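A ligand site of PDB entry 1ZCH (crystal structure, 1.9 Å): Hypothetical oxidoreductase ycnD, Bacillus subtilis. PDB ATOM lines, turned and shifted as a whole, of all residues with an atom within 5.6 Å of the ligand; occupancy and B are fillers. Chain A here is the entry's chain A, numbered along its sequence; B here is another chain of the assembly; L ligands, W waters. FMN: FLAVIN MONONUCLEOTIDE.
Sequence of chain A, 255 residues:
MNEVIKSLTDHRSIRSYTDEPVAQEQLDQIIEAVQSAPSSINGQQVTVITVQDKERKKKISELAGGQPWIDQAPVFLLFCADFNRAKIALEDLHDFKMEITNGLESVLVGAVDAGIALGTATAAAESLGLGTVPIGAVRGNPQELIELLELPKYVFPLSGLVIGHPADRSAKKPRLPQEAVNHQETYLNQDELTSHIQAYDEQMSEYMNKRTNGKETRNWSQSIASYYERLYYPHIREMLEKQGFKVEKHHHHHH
N10 of the ligand sits close to O of Pro 134 (3.4 Å). Arg 12 touches the ligand. Trp 69 touches the ligand (CZ2 to O2, 3.4 Å). Val 133 touches the ligand (CG2 to N1, 3.6 Å). Ile 135 touches the ligand (CA to O4, 3.5 Å). Ala 137 touches the ligand. Ser 159 touches the ligand. Pro 38 of chain B touches the ligand. Ser 40 of chain B touches the ligand. Asn 42 of chain B touches the ligand (CB to O4', 3.3 Å). CG1 of Val 112 of chain B touches C7M of the ligand, 3.9 Å away. Ile 116 of chain B touches the ligand. Of the 27 residues printed, 20 come within 4 Å of the ligand.
Water W7 lies within hydrogen-bond range of O1P of the ligand, N of Lys 173 and O of His 11. Water W5 lies within hydrogen-bond range of O2P of the ligand (2.8 Å), NH1 of Arg 15 (3.0 Å) and NZ of Lys 173 (3.2 Å). Water W2 bridges the backbone carbonyl oxygen of Ala 171 and an oxygen (O2P) of the ligand. Water W1 bridges N5 of the ligand (3.3 Å) and OG of Ser 40 of chain B (3.3 Å).
NH2 of Arg 175 lies within salt-bridge range of O1P of the ligand. An oxygen (O3') of the ligand lies within hydrogen-bond range of the backbone NH (N) of Ser 39 of chain B (3.4 Å). OE1 of Gln 67 lies within hydrogen-bond range of N3 of the ligand (2.7 Å). A ring nitrogen (NE2) of His 11 sits at hydrogen-bond distance from an oxygen (O3P) of the ligand, 3.0 Å away. O3' of the ligand is in hydrogen-bond range of O of Ser 39 of chain B, 3.4 Å away. An oxygen (O4') of the ligand sits at hydrogen-bond distance from the side-chain amino group (NZ) of Lys 173 (2.7 Å). O3P of the ligand is in hydrogen-bond range of OG of Ser 13 (2.7 Å). NE of Arg 15 is in hydrogen-bond range of O2 of the ligand (2.7 Å). A nitrogen (N5) of the ligand sits at hydrogen-bond distance from the backbone NH (N) of Gly 136, 2.7 Å away. The backbone NH (N) of Ser 13 sits at hydrogen-bond distance from an oxygen (O2P) of the ligand, 2.7 Å away.
NH2 of Arg 175 lies within hydrogen-bond range of O of Ala 37 of chain B, at 3.0 Å. The guanidinium group (NH2) of Arg 175 is in hydrogen-bond range of the backbone carbonyl oxygen (O) of Ser 36 of chain B (3.2 Å). OE1 of Gln 67 sits at hydrogen-bond distance from NE1 of Trp 69. The side-chain carboxylate (OD1) of Asp 113 of chain B lies within hydrogen-bond range of the backbone NH (N) of Ser 40 of chain B (3.1 Å). NH1 of Arg 175 is in hydrogen-bond range of O of Lys 173, 3.0 Å away.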
ATOM      1  N   HIS A  11      -4.321  -0.482 -16.111  1.00  0.00           N
ATOM      2  CA  HIS A  11      -4.335  -0.401 -14.652  1.00  0.00           C
ATOM      3  C   HIS A  11      -5.244  -1.371 -13.894  1.00  0.00           C
ATOM      4  O   HIS A  11      -6.359  -1.661 -14.323  1.00  0.00           O
ATOM      5  CB  HIS A  11      -4.714   1.011 -14.183  1.00  0.00           C
ATOM      6  CG  HIS A  11      -5.043   1.080 -12.730  1.00  0.00           C
ATOM      7  ND1 HIS A  11      -4.076   1.103 -11.745  1.00  0.00           N
ATOM      8  CD2 HIS A  11      -6.232   0.996 -12.074  1.00  0.00           C
ATOM      9  CE1 HIS A  11      -4.641   1.034 -10.556  1.00  0.00           C
ATOM     10  NE2 HIS A  11      -5.953   0.968 -10.724  1.00  0.00           N
ATOM     11  N   ARG A  12      -4.743  -1.843 -12.756  1.00  0.00           N
ATOM     12  CA  ARG A  12      -5.490  -2.701 -11.833  1.00  0.00           C
ATOM     13  C   ARG A  12      -4.729  -2.622 -10.511  1.00  0.00           C
ATOM     14  O   ARG A  12      -3.503  -2.584 -10.493  1.00  0.00           O
ATOM     15  CB  ARG A  12      -5.578  -4.162 -12.311  1.00  0.00           C
ATOM     16  CG  ARG A  12      -4.380  -5.065 -11.997  1.00  0.00           C
ATOM     17  CD  ARG A  12      -3.181  -4.689 -12.842  1.00  0.00           C
ATOM     18  NE  ARG A  12      -3.505  -4.718 -14.264  1.00  0.00           N
ATOM     19  CZ  ARG A  12      -3.733  -5.813 -14.967  1.00  0.00           C
ATOM     20  NH1 ARG A  12      -3.679  -7.006 -14.389  1.00  0.00           N
ATOM     21  NH2 ARG A  12      -4.015  -5.733 -16.265  1.00  0.00           N
ATOM     22  N   SER A  13      -5.458  -2.554  -9.406  1.00  0.00           N
ATOM     23  CA  SER A  13      -4.825  -2.477  -8.100  1.00  0.00           C
ATOM     24  C   SER A  13      -4.225  -3.816  -7.691  1.00  0.00           C
ATOM     25  O   SER A  13      -4.807  -4.876  -7.953  1.00  0.00           O
ATOM     26  CB  SER A  13      -5.833  -2.026  -7.032  1.00  0.00           C
ATOM     27  OG  SER A  13      -6.110  -0.638  -7.171  1.00  0.00           O
ATOM     28  N   ARG A  15      -2.755  -6.150  -4.507  1.00  0.00           N
ATOM     29  CA  ARG A  15      -2.806  -6.289  -3.049  1.00  0.00           C
ATOM     30  C   ARG A  15      -2.000  -7.482  -2.531  1.00  0.00           C
ATOM     31  O   ARG A  15      -2.127  -7.882  -1.376  1.00  0.00           O
ATOM     32  CB  ARG A  15      -4.260  -6.405  -2.573  1.00  0.00           C
ATOM     33  CG  ARG A  15      -5.089  -5.166  -2.855  1.00  0.00           C
ATOM     34  CD  ARG A  15      -6.466  -5.258  -2.218  1.00  0.00           C
ATOM     35  NE  ARG A  15      -7.262  -4.059  -2.494  1.00  0.00           N
ATOM     36  CZ  ARG A  15      -7.901  -3.823  -3.633  1.00  0.00           C
ATOM     37  NH1 ARG A  15      -7.850  -4.713  -4.623  1.00  0.00           N
ATOM     38  NH2 ARG A  15      -8.586  -2.700  -3.790  1.00  0.00           N
ATOM     39  N   GLN A  67      -4.781  -3.563   6.946  1.00  0.00           N
ATOM     40  CA  GLN A  67      -4.759  -4.054   5.575  1.00  0.00           C
ATOM     41  C   GLN A  67      -3.369  -4.644   5.343  1.00  0.00           C
ATOM     42  O   GLN A  67      -2.382  -3.919   5.194  1.00  0.00           O
ATOM     43  CB  GLN A  67      -5.054  -2.909   4.609  1.00  0.00           C
ATOM     44  CG  GLN A  67      -6.428  -2.291   4.838  1.00  0.00           C
ATOM     45  CD  GLN A  67      -6.818  -1.272   3.783  1.00  0.00           C
ATOM     46  OE1 GLN A  67      -6.746  -1.561   2.588  1.00  0.00           O
ATOM     47  NE2 GLN A  67      -7.257  -0.097   4.215  1.00  0.00           N
ATOM     48  N   TRP A  69      -1.608  -5.807   2.886  1.00  0.00           N
ATOM     49  CA  TRP A  69      -0.745  -5.384   1.787  1.00  0.00           C
ATOM     50  C   TRP A  69       0.126  -4.172   2.150  1.00  0.00           C
ATOM     51  O   TRP A  69       1.176  -3.973   1.555  1.00  0.00           O
ATOM     52  CB  TRP A  69      -1.574  -5.114   0.532  1.00  0.00           C
ATOM     53  CG  TRP A  69      -2.925  -4.518   0.779  1.00  0.00           C
ATOM     54  CD1 TRP A  69      -3.255  -3.194   0.819  1.00  0.00           C
ATOM     55  CD2 TRP A  69      -4.149  -5.238   1.001  1.00  0.00           C
ATOM     56  NE1 TRP A  69      -4.601  -3.045   1.046  1.00  0.00           N
ATOM     57  CE2 TRP A  69      -5.169  -4.291   1.169  1.00  0.00           C
ATOM     58  CE3 TRP A  69      -4.467  -6.601   1.084  1.00  0.00           C
ATOM     59  CZ2 TRP A  69      -6.497  -4.647   1.408  1.00  0.00           C
ATOM     60  CZ3 TRP A  69      -5.789  -6.962   1.315  1.00  0.00           C
ATOM     61  CH2 TRP A  69      -6.794  -5.987   1.480  1.00  0.00           C
ATOM     62  N   LEU A 118      -1.718  11.664  -6.568  1.00  0.00           N
ATOM     63  CA  LEU A 118      -1.936  10.222  -6.416  1.00  0.00           C
ATOM     64  C   LEU A 118      -2.092   9.533  -7.773  1.00  0.00           C
ATOM     65  O   LEU A 118      -1.494   8.478  -8.020  1.00  0.00           O
ATOM     66  CB  LEU A 118      -3.181   9.983  -5.561  1.00  0.00           C
ATOM     67  CG  LEU A 118      -3.611   8.549  -5.274  1.00  0.00           C
ATOM     68  CD1 LEU A 118      -2.605   7.881  -4.351  1.00  0.00           C
ATOM     69  CD2 LEU A 118      -4.989   8.550  -4.621  1.00  0.00           C
ATOM     70  N   VAL A 133      -1.778   0.314  -4.843  1.00  0.00           N
ATOM     71  CA  VAL A 133      -3.166   0.326  -4.387  1.00  0.00           C
ATOM     72  C   VAL A 133      -3.310   1.506  -3.427  1.00  0.00           C
ATOM     73  O   VAL A 133      -2.556   1.636  -2.464  1.00  0.00           O
ATOM     74  CB  VAL A 133      -3.592  -0.992  -3.672  1.00  0.00           C
ATOM     75  CG1 VAL A 133      -2.841  -1.190  -2.368  1.00  0.00           C
ATOM     76  CG2 VAL A 133      -5.104  -0.955  -3.429  1.00  0.00           C
ATOM     77  N   PRO A 134      -4.244   2.420  -3.719  1.00  0.00           N
ATOM     78  CA  PRO A 134      -4.408   3.571  -2.828  1.00  0.00           C
ATOM     79  C   PRO A 134      -5.050   3.102  -1.526  1.00  0.00           C
ATOM     80  O   PRO A 134      -5.657   2.037  -1.482  1.00  0.00           O
ATOM     81  CB  PRO A 134      -5.332   4.505  -3.615  1.00  0.00           C
ATOM     82  CG  PRO A 134      -5.128   4.092  -5.054  1.00  0.00           C
ATOM     83  CD  PRO A 134      -5.050   2.587  -4.938  1.00  0.00           C
ATOM     84  N   ILE A 135      -4.908   3.907  -0.473  1.00  0.00           N
ATOM     85  CA  ILE A 135      -5.473   3.571   0.829  1.00  0.00           C
ATOM     86  C   ILE A 135      -6.235   4.773   1.394  1.00  0.00           C
ATOM     87  O   ILE A 135      -5.645   5.629   2.046  1.00  0.00           O
ATOM     88  CB  ILE A 135      -4.380   3.150   1.834  1.00  0.00           C
ATOM     89  CG1 ILE A 135      -3.616   1.919   1.315  1.00  0.00           C
ATOM     90  CG2 ILE A 135      -5.010   2.854   3.201  1.00  0.00           C
ATOM     91  CD1 ILE A 135      -4.450   0.646   1.242  1.00  0.00           C
ATOM     92  N   GLY A 136      -7.541   4.812   1.155  1.00  0.00           N
ATOM     93  CA  GLY A 136      -8.334   5.925   1.662  1.00  0.00           C
ATOM     94  C   GLY A 136      -8.605   5.789   3.140  1.00  0.00           C
ATOM     95  O   GLY A 136      -9.013   6.747   3.791  1.00  0.00           O
ATOM     96  N   ALA A 137      -8.377   4.588   3.677  1.00  0.00           N
ATOM     97  CA  ALA A 137      -8.621   4.311   5.089  1.00  0.00           C
ATOM     98  C   ALA A 137      -7.732   5.112   6.040  1.00  0.00           C
ATOM     99  O   ALA A 137      -7.908   5.053   7.254  1.00  0.00           O
ATOM    100  CB  ALA A 137      -8.452   2.826   5.365  1.00  0.00           C
ATOM    101  N   ARG A 139      -7.950   8.003   6.445  1.00  0.00           N
ATOM    102  CA  ARG A 139      -8.838   9.010   7.008  1.00  0.00           C
ATOM    103  C   ARG A 139      -9.696   8.447   8.150  1.00  0.00           C
ATOM    104  O   ARG A 139     -10.500   9.164   8.737  1.00  0.00           O
ATOM    105  CB  ARG A 139      -9.755   9.591   5.911  1.00  0.00           C
ATOM    106  CG  ARG A 139      -8.997  10.285   4.783  1.00  0.00           C
ATOM    107  CD  ARG A 139      -9.856  11.361   4.107  1.00  0.00           C
ATOM    108  NE  ARG A 139     -10.974  10.817   3.329  1.00  0.00           N
ATOM    109  CZ  ARG A 139     -10.903  10.495   2.040  1.00  0.00           C
ATOM    110  NH1 ARG A 139      -9.770  10.666   1.373  1.00  0.00           N
ATOM    111  NH2 ARG A 139     -11.972  10.032   1.410  1.00  0.00           N
ATOM    112  N   SER A 159      -4.888  10.255   1.303  1.00  0.00           N
ATOM    113  CA  SER A 159      -4.810   8.874   0.842  1.00  0.00           C
ATOM    114  C   SER A 159      -3.388   8.340   0.827  1.00  0.00           C
ATOM    115  O   SER A 159      -2.440   9.069   0.533  1.00  0.00           O
ATOM    116  CB  SER A 159      -5.406   8.743  -0.557  1.00  0.00           C
ATOM    117  OG  SER A 159      -5.355   7.398  -1.033  1.00  0.00           O
ATOM    118  N   ALA A 171      -6.266  -8.909 -12.103  1.00  0.00           N
ATOM    119  CA  ALA A 171      -6.944  -8.674 -13.371  1.00  0.00           C
ATOM    120  C   ALA A 171      -7.731  -7.367 -13.336  1.00  0.00           C
ATOM    121  O   ALA A 171      -8.051  -6.844 -12.264  1.00  0.00           O
ATOM    122  CB  ALA A 171      -7.874  -9.827 -13.675  1.00  0.00           C
ATOM    123  N   LYS A 173     -10.752  -4.763 -13.505  1.00  0.00           N
ATOM    124  CA  LYS A 173     -12.130  -4.753 -13.013  1.00  0.00           C
ATOM    125  C   LYS A 173     -12.989  -3.871 -13.928  1.00  0.00           C
ATOM    126  O   LYS A 173     -12.627  -2.734 -14.210  1.00  0.00           O
ATOM    127  CB  LYS A 173     -12.147  -4.210 -11.584  1.00  0.00           C
ATOM    128  CG  LYS A 173     -13.507  -4.199 -10.922  1.00  0.00           C
ATOM    129  CD  LYS A 173     -13.434  -3.518  -9.558  1.00  0.00           C
ATOM    130  CE  LYS A 173     -12.406  -4.179  -8.663  1.00  0.00           C
ATOM    131  NZ  LYS A 173     -12.398  -3.589  -7.297  1.00  0.00           N
ATOM    132  N   ARG A 175     -15.534  -1.315 -15.656  1.00  0.00           N
ATOM    133  CA  ARG A 175     -15.905   0.047 -15.292  1.00  0.00           C
ATOM    134  C   ARG A 175     -17.254   0.369 -15.912  1.00  0.00           C
ATOM    135  O   ARG A 175     -17.714  -0.319 -16.824  1.00  0.00           O
ATOM    136  CB  ARG A 175     -14.867   1.049 -15.827  1.00  0.00           C
ATOM    137  CG  ARG A 175     -13.459   0.882 -15.250  1.00  0.00           C
ATOM    138  CD  ARG A 175     -13.453   1.173 -13.769  1.00  0.00           C
ATOM    139  NE  ARG A 175     -12.113   1.508 -13.284  1.00  0.00           N
ATOM    140  CZ  ARG A 175     -11.303   0.669 -12.628  1.00  0.00           C
ATOM    141  NH1 ARG A 175     -11.666  -0.583 -12.393  1.00  0.00           N
ATOM    142  NH2 ARG A 175     -10.122   1.105 -12.202  1.00  0.00           N
ATOM    143  N   SER B  36     -10.097   4.050 -16.508  1.00  0.00           N
ATOM    144  CA  SER B  36      -9.236   2.959 -16.060  1.00  0.00           C
ATOM    145  C   SER B  36      -8.471   3.227 -14.760  1.00  0.00           C
ATOM    146  O   SER B  36      -7.948   2.301 -14.144  1.00  0.00           O
ATOM    147  CB  SER B  36      -8.250   2.589 -17.165  1.00  0.00           C
ATOM    148  OG  SER B  36      -8.925   2.149 -18.322  1.00  0.00           O
ATOM    149  N   ALA B  37      -8.402   4.492 -14.353  1.00  0.00           N
ATOM    150  CA  ALA B  37      -7.704   4.851 -13.130  1.00  0.00           C
ATOM    151  C   ALA B  37      -8.472   4.394 -11.894  1.00  0.00           C
ATOM    152  O   ALA B  37      -9.668   4.100 -11.965  1.00  0.00           O
ATOM    153  CB  ALA B  37      -7.494   6.368 -13.079  1.00  0.00           C
ATOM    154  N   PRO B  38      -7.803   4.329 -10.745  1.00  0.00           N
ATOM    155  CA  PRO B  38      -8.485   3.889  -9.520  1.00  0.00           C
ATOM    156  C   PRO B  38      -9.487   4.915  -8.990  1.00  0.00           C
ATOM    157  O   PRO B  38      -9.418   6.100  -9.337  1.00  0.00           O
ATOM    158  CB  PRO B  38      -7.326   3.645  -8.550  1.00  0.00           C
ATOM    159  CG  PRO B  38      -6.326   4.696  -8.974  1.00  0.00           C
ATOM    160  CD  PRO B  38      -6.368   4.588 -10.491  1.00  0.00           C
ATOM    161  N   SER B  39     -10.420   4.445  -8.172  1.00  0.00           N
ATOM    162  CA  SER B  39     -11.419   5.316  -7.550  1.00  0.00           C
ATOM    163  C   SER B  39     -11.825   4.644  -6.237  1.00  0.00           C
ATOM    164  O   SER B  39     -11.808   3.428  -6.125  1.00  0.00           O
ATOM    165  CB  SER B  39     -12.643   5.503  -8.454  1.00  0.00           C
ATOM    166  OG  SER B  39     -13.422   4.316  -8.547  1.00  0.00           O
ATOM    167  N   SER B  40     -12.169   5.446  -5.233  1.00  0.00           N
ATOM    168  CA  SER B  40     -12.549   4.913  -3.937  1.00  0.00           C
ATOM    169  C   SER B  40     -13.706   3.906  -4.071  1.00  0.00           C
ATOM    170  O   SER B  40     -14.741   4.231  -4.651  1.00  0.00           O
ATOM    171  CB  SER B  40     -12.934   6.056  -2.994  1.00  0.00           C
ATOM    172  OG  SER B  40     -13.074   5.601  -1.664  1.00  0.00           O
ATOM    173  N   ILE B  41     -13.484   2.709  -3.526  1.00  0.00           N
ATOM    174  CA  ILE B  41     -14.429   1.575  -3.572  1.00  0.00           C
ATOM    175  C   ILE B  41     -14.985   1.311  -4.974  1.00  0.00           C
ATOM    176  O   ILE B  41     -16.084   0.771  -5.135  1.00  0.00           O
ATOM    177  CB  ILE B  41     -15.631   1.746  -2.581  1.00  0.00           C
ATOM    178  CG1 ILE B  41     -16.615   2.808  -3.083  1.00  0.00           C
ATOM    179  CG2 ILE B  41     -15.112   2.112  -1.197  1.00  0.00           C
ATOM    180  CD1 ILE B  41     -17.908   2.843  -2.297  1.00  0.00           C
ATOM    181  N   ASN B  42     -14.203   1.667  -5.987  1.00  0.00           N
ATOM    182  CA  ASN B  42     -14.605   1.524  -7.391  1.00  0.00           C
ATOM    183  C   ASN B  42     -15.917   2.268  -7.593  1.00  0.00           C
ATOM    184  O   ASN B  42     -16.719   1.933  -8.463  1.00  0.00           O
ATOM    185  CB  ASN B  42     -14.772   0.049  -7.784  1.00  0.00           C
ATOM    186  CG  ASN B  42     -14.933  -0.133  -9.297  1.00  0.00           C
ATOM    187  OD1 ASN B  42     -14.318   0.578 -10.086  1.00  0.00           O
ATOM    188  ND2 ASN B  42     -15.761  -1.097  -9.698  1.00  0.00           N
ATOM    189  N   VAL B 112     -10.968  13.911  -4.479  1.00  0.00           N
ATOM    190  CA  VAL B 112      -9.801  13.082  -4.752  1.00  0.00           C
ATOM    191  C   VAL B 112     -10.020  12.264  -6.029  1.00  0.00           C
ATOM    192  O   VAL B 112      -9.111  12.144  -6.861  1.00  0.00           O
ATOM    193  CB  VAL B 112      -9.484  12.138  -3.574  1.00  0.00           C
ATOM    194  CG1 VAL B 112      -8.356  11.151  -3.956  1.00  0.00           C
ATOM    195  CG2 VAL B 112      -9.070  12.955  -2.365  1.00  0.00           C
ATOM    196  N   ASP B 113     -11.214  11.704  -6.197  1.00  0.00           N
ATOM    197  CA  ASP B 113     -11.493  10.918  -7.400  1.00  0.00           C
ATOM    198  C   ASP B 113     -11.353  11.840  -8.621  1.00  0.00           C
ATOM    199  O   ASP B 113     -10.774  11.452  -9.633  1.00  0.00           O
ATOM    200  CB  ASP B 113     -12.924  10.336  -7.352  1.00  0.00           C
ATOM    201  CG  ASP B 113     -12.973   8.916  -6.755  1.00  0.00           C
ATOM    202  OD1 ASP B 113     -11.992   8.454  -6.139  1.00  0.00           O
ATOM    203  OD2 ASP B 113     -14.032   8.261  -6.901  1.00  0.00           O
ATOM    204  N   ILE B 116      -7.696  12.593  -9.373  1.00  0.00           N
ATOM    205  CA  ILE B 116      -7.069  11.448 -10.009  1.00  0.00           C
ATOM    206  C   ILE B 116      -7.450  11.459 -11.487  1.00  0.00           C
ATOM    207  O   ILE B 116      -6.618  11.244 -12.368  1.00  0.00           O
ATOM    208  CB  ILE B 116      -7.553  10.127  -9.382  1.00  0.00           C
ATOM    209  CG1 ILE B 116      -6.954   9.971  -7.984  1.00  0.00           C
ATOM    210  CG2 ILE B 116      -7.195   8.932 -10.274  1.00  0.00           C
ATOM    211  CD1 ILE B 116      -7.530   8.805  -7.209  1.00  0.00           C
HETATM  212  N1  FMN L   1      -8.229  -0.382  -1.793  1.00  0.00           N
HETATM  213  C2  FMN L   1      -8.001  -1.006  -0.618  1.00  0.00           C
HETATM  214  O2  FMN L   1      -7.767  -2.179  -0.555  1.00  0.00           O
HETATM  215  N3  FMN L   1      -8.016  -0.297   0.632  1.00  0.00           N
HETATM  216  C4  FMN L   1      -8.263   1.078   0.695  1.00  0.00           C
HETATM  217  O4  FMN L   1      -8.268   1.636   1.773  1.00  0.00           O
HETATM  218  C4A FMN L   1      -8.496   1.781  -0.571  1.00  0.00           C
HETATM  219  N5  FMN L   1      -8.747   3.130  -0.582  1.00  0.00           N
HETATM  220  C5A FMN L   1      -8.787   3.774  -1.801  1.00  0.00           C
HETATM  221  C6  FMN L   1      -8.855   5.213  -1.786  1.00  0.00           C
HETATM  222  C7  FMN L   1      -8.848   5.956  -2.968  1.00  0.00           C
HETATM  223  C7M FMN L   1      -8.855   7.462  -2.901  1.00  0.00           C
HETATM  224  C8  FMN L   1      -8.802   5.262  -4.272  1.00  0.00           C
HETATM  225  C8M FMN L   1      -8.740   6.015  -5.570  1.00  0.00           C
HETATM  226  C9  FMN L   1      -8.769   3.837  -4.308  1.00  0.00           C
HETATM  227  C9A FMN L   1      -8.747   3.085  -3.098  1.00  0.00           C
HETATM  228  N10 FMN L   1      -8.615   1.623  -3.034  1.00  0.00           N
HETATM  229  C10 FMN L   1      -8.459   0.974  -1.832  1.00  0.00           C
HETATM  230  C1' FMN L   1      -8.602   0.838  -4.313  1.00  0.00           C
HETATM  231  C2' FMN L   1     -10.037   0.679  -4.934  1.00  0.00           C
HETATM  232  O2' FMN L   1     -10.722  -0.346  -4.217  1.00  0.00           O
HETATM  233  C3' FMN L   1      -9.860   0.312  -6.421  1.00  0.00           C
HETATM  234  O3' FMN L   1      -9.198   1.419  -7.078  1.00  0.00           O
HETATM  235  C4' FMN L   1     -11.219   0.076  -7.106  1.00  0.00           C
HETATM  236  O4' FMN L   1     -11.890  -1.064  -6.549  1.00  0.00           O
HETATM  237  C5' FMN L   1     -10.974  -0.114  -8.598  1.00  0.00           C
HETATM  238  O5' FMN L   1     -10.195  -1.450  -8.847  1.00  0.00           O
HETATM  239  P   FMN L   1      -8.839  -1.343  -9.552  1.00  0.00           P
HETATM  240  O1P FMN L   1      -9.049  -1.096 -10.972  1.00  0.00           O
HETATM  241  O2P FMN L   1      -8.146  -2.609  -9.390  1.00  0.00           O
HETATM  242  O3P FMN L   1      -8.041  -0.269  -8.985  1.00  0.00           O
HETATM  243  O   HOH W   1     -11.884   3.344   0.493  1.00  0.00           O
HETATM  244  O   HOH W   2      -8.878  -5.190 -10.257  1.00  0.00           O
HETATM  245  O   HOH W   3     -10.816   9.351  -1.093  1.00  0.00           O
HETATM  246  O   HOH W   4     -11.579   9.334  -3.759  1.00  0.00           O
HETATM  247  O   HOH W   5      -9.212  -3.834  -7.120  1.00  0.00           O
HETATM  248  O   HOH W   6     -11.254   6.809  -0.005  1.00  0.00           O
HETATM  249  O   HOH W   7      -8.832  -2.801 -13.017  1.00  0.00           O
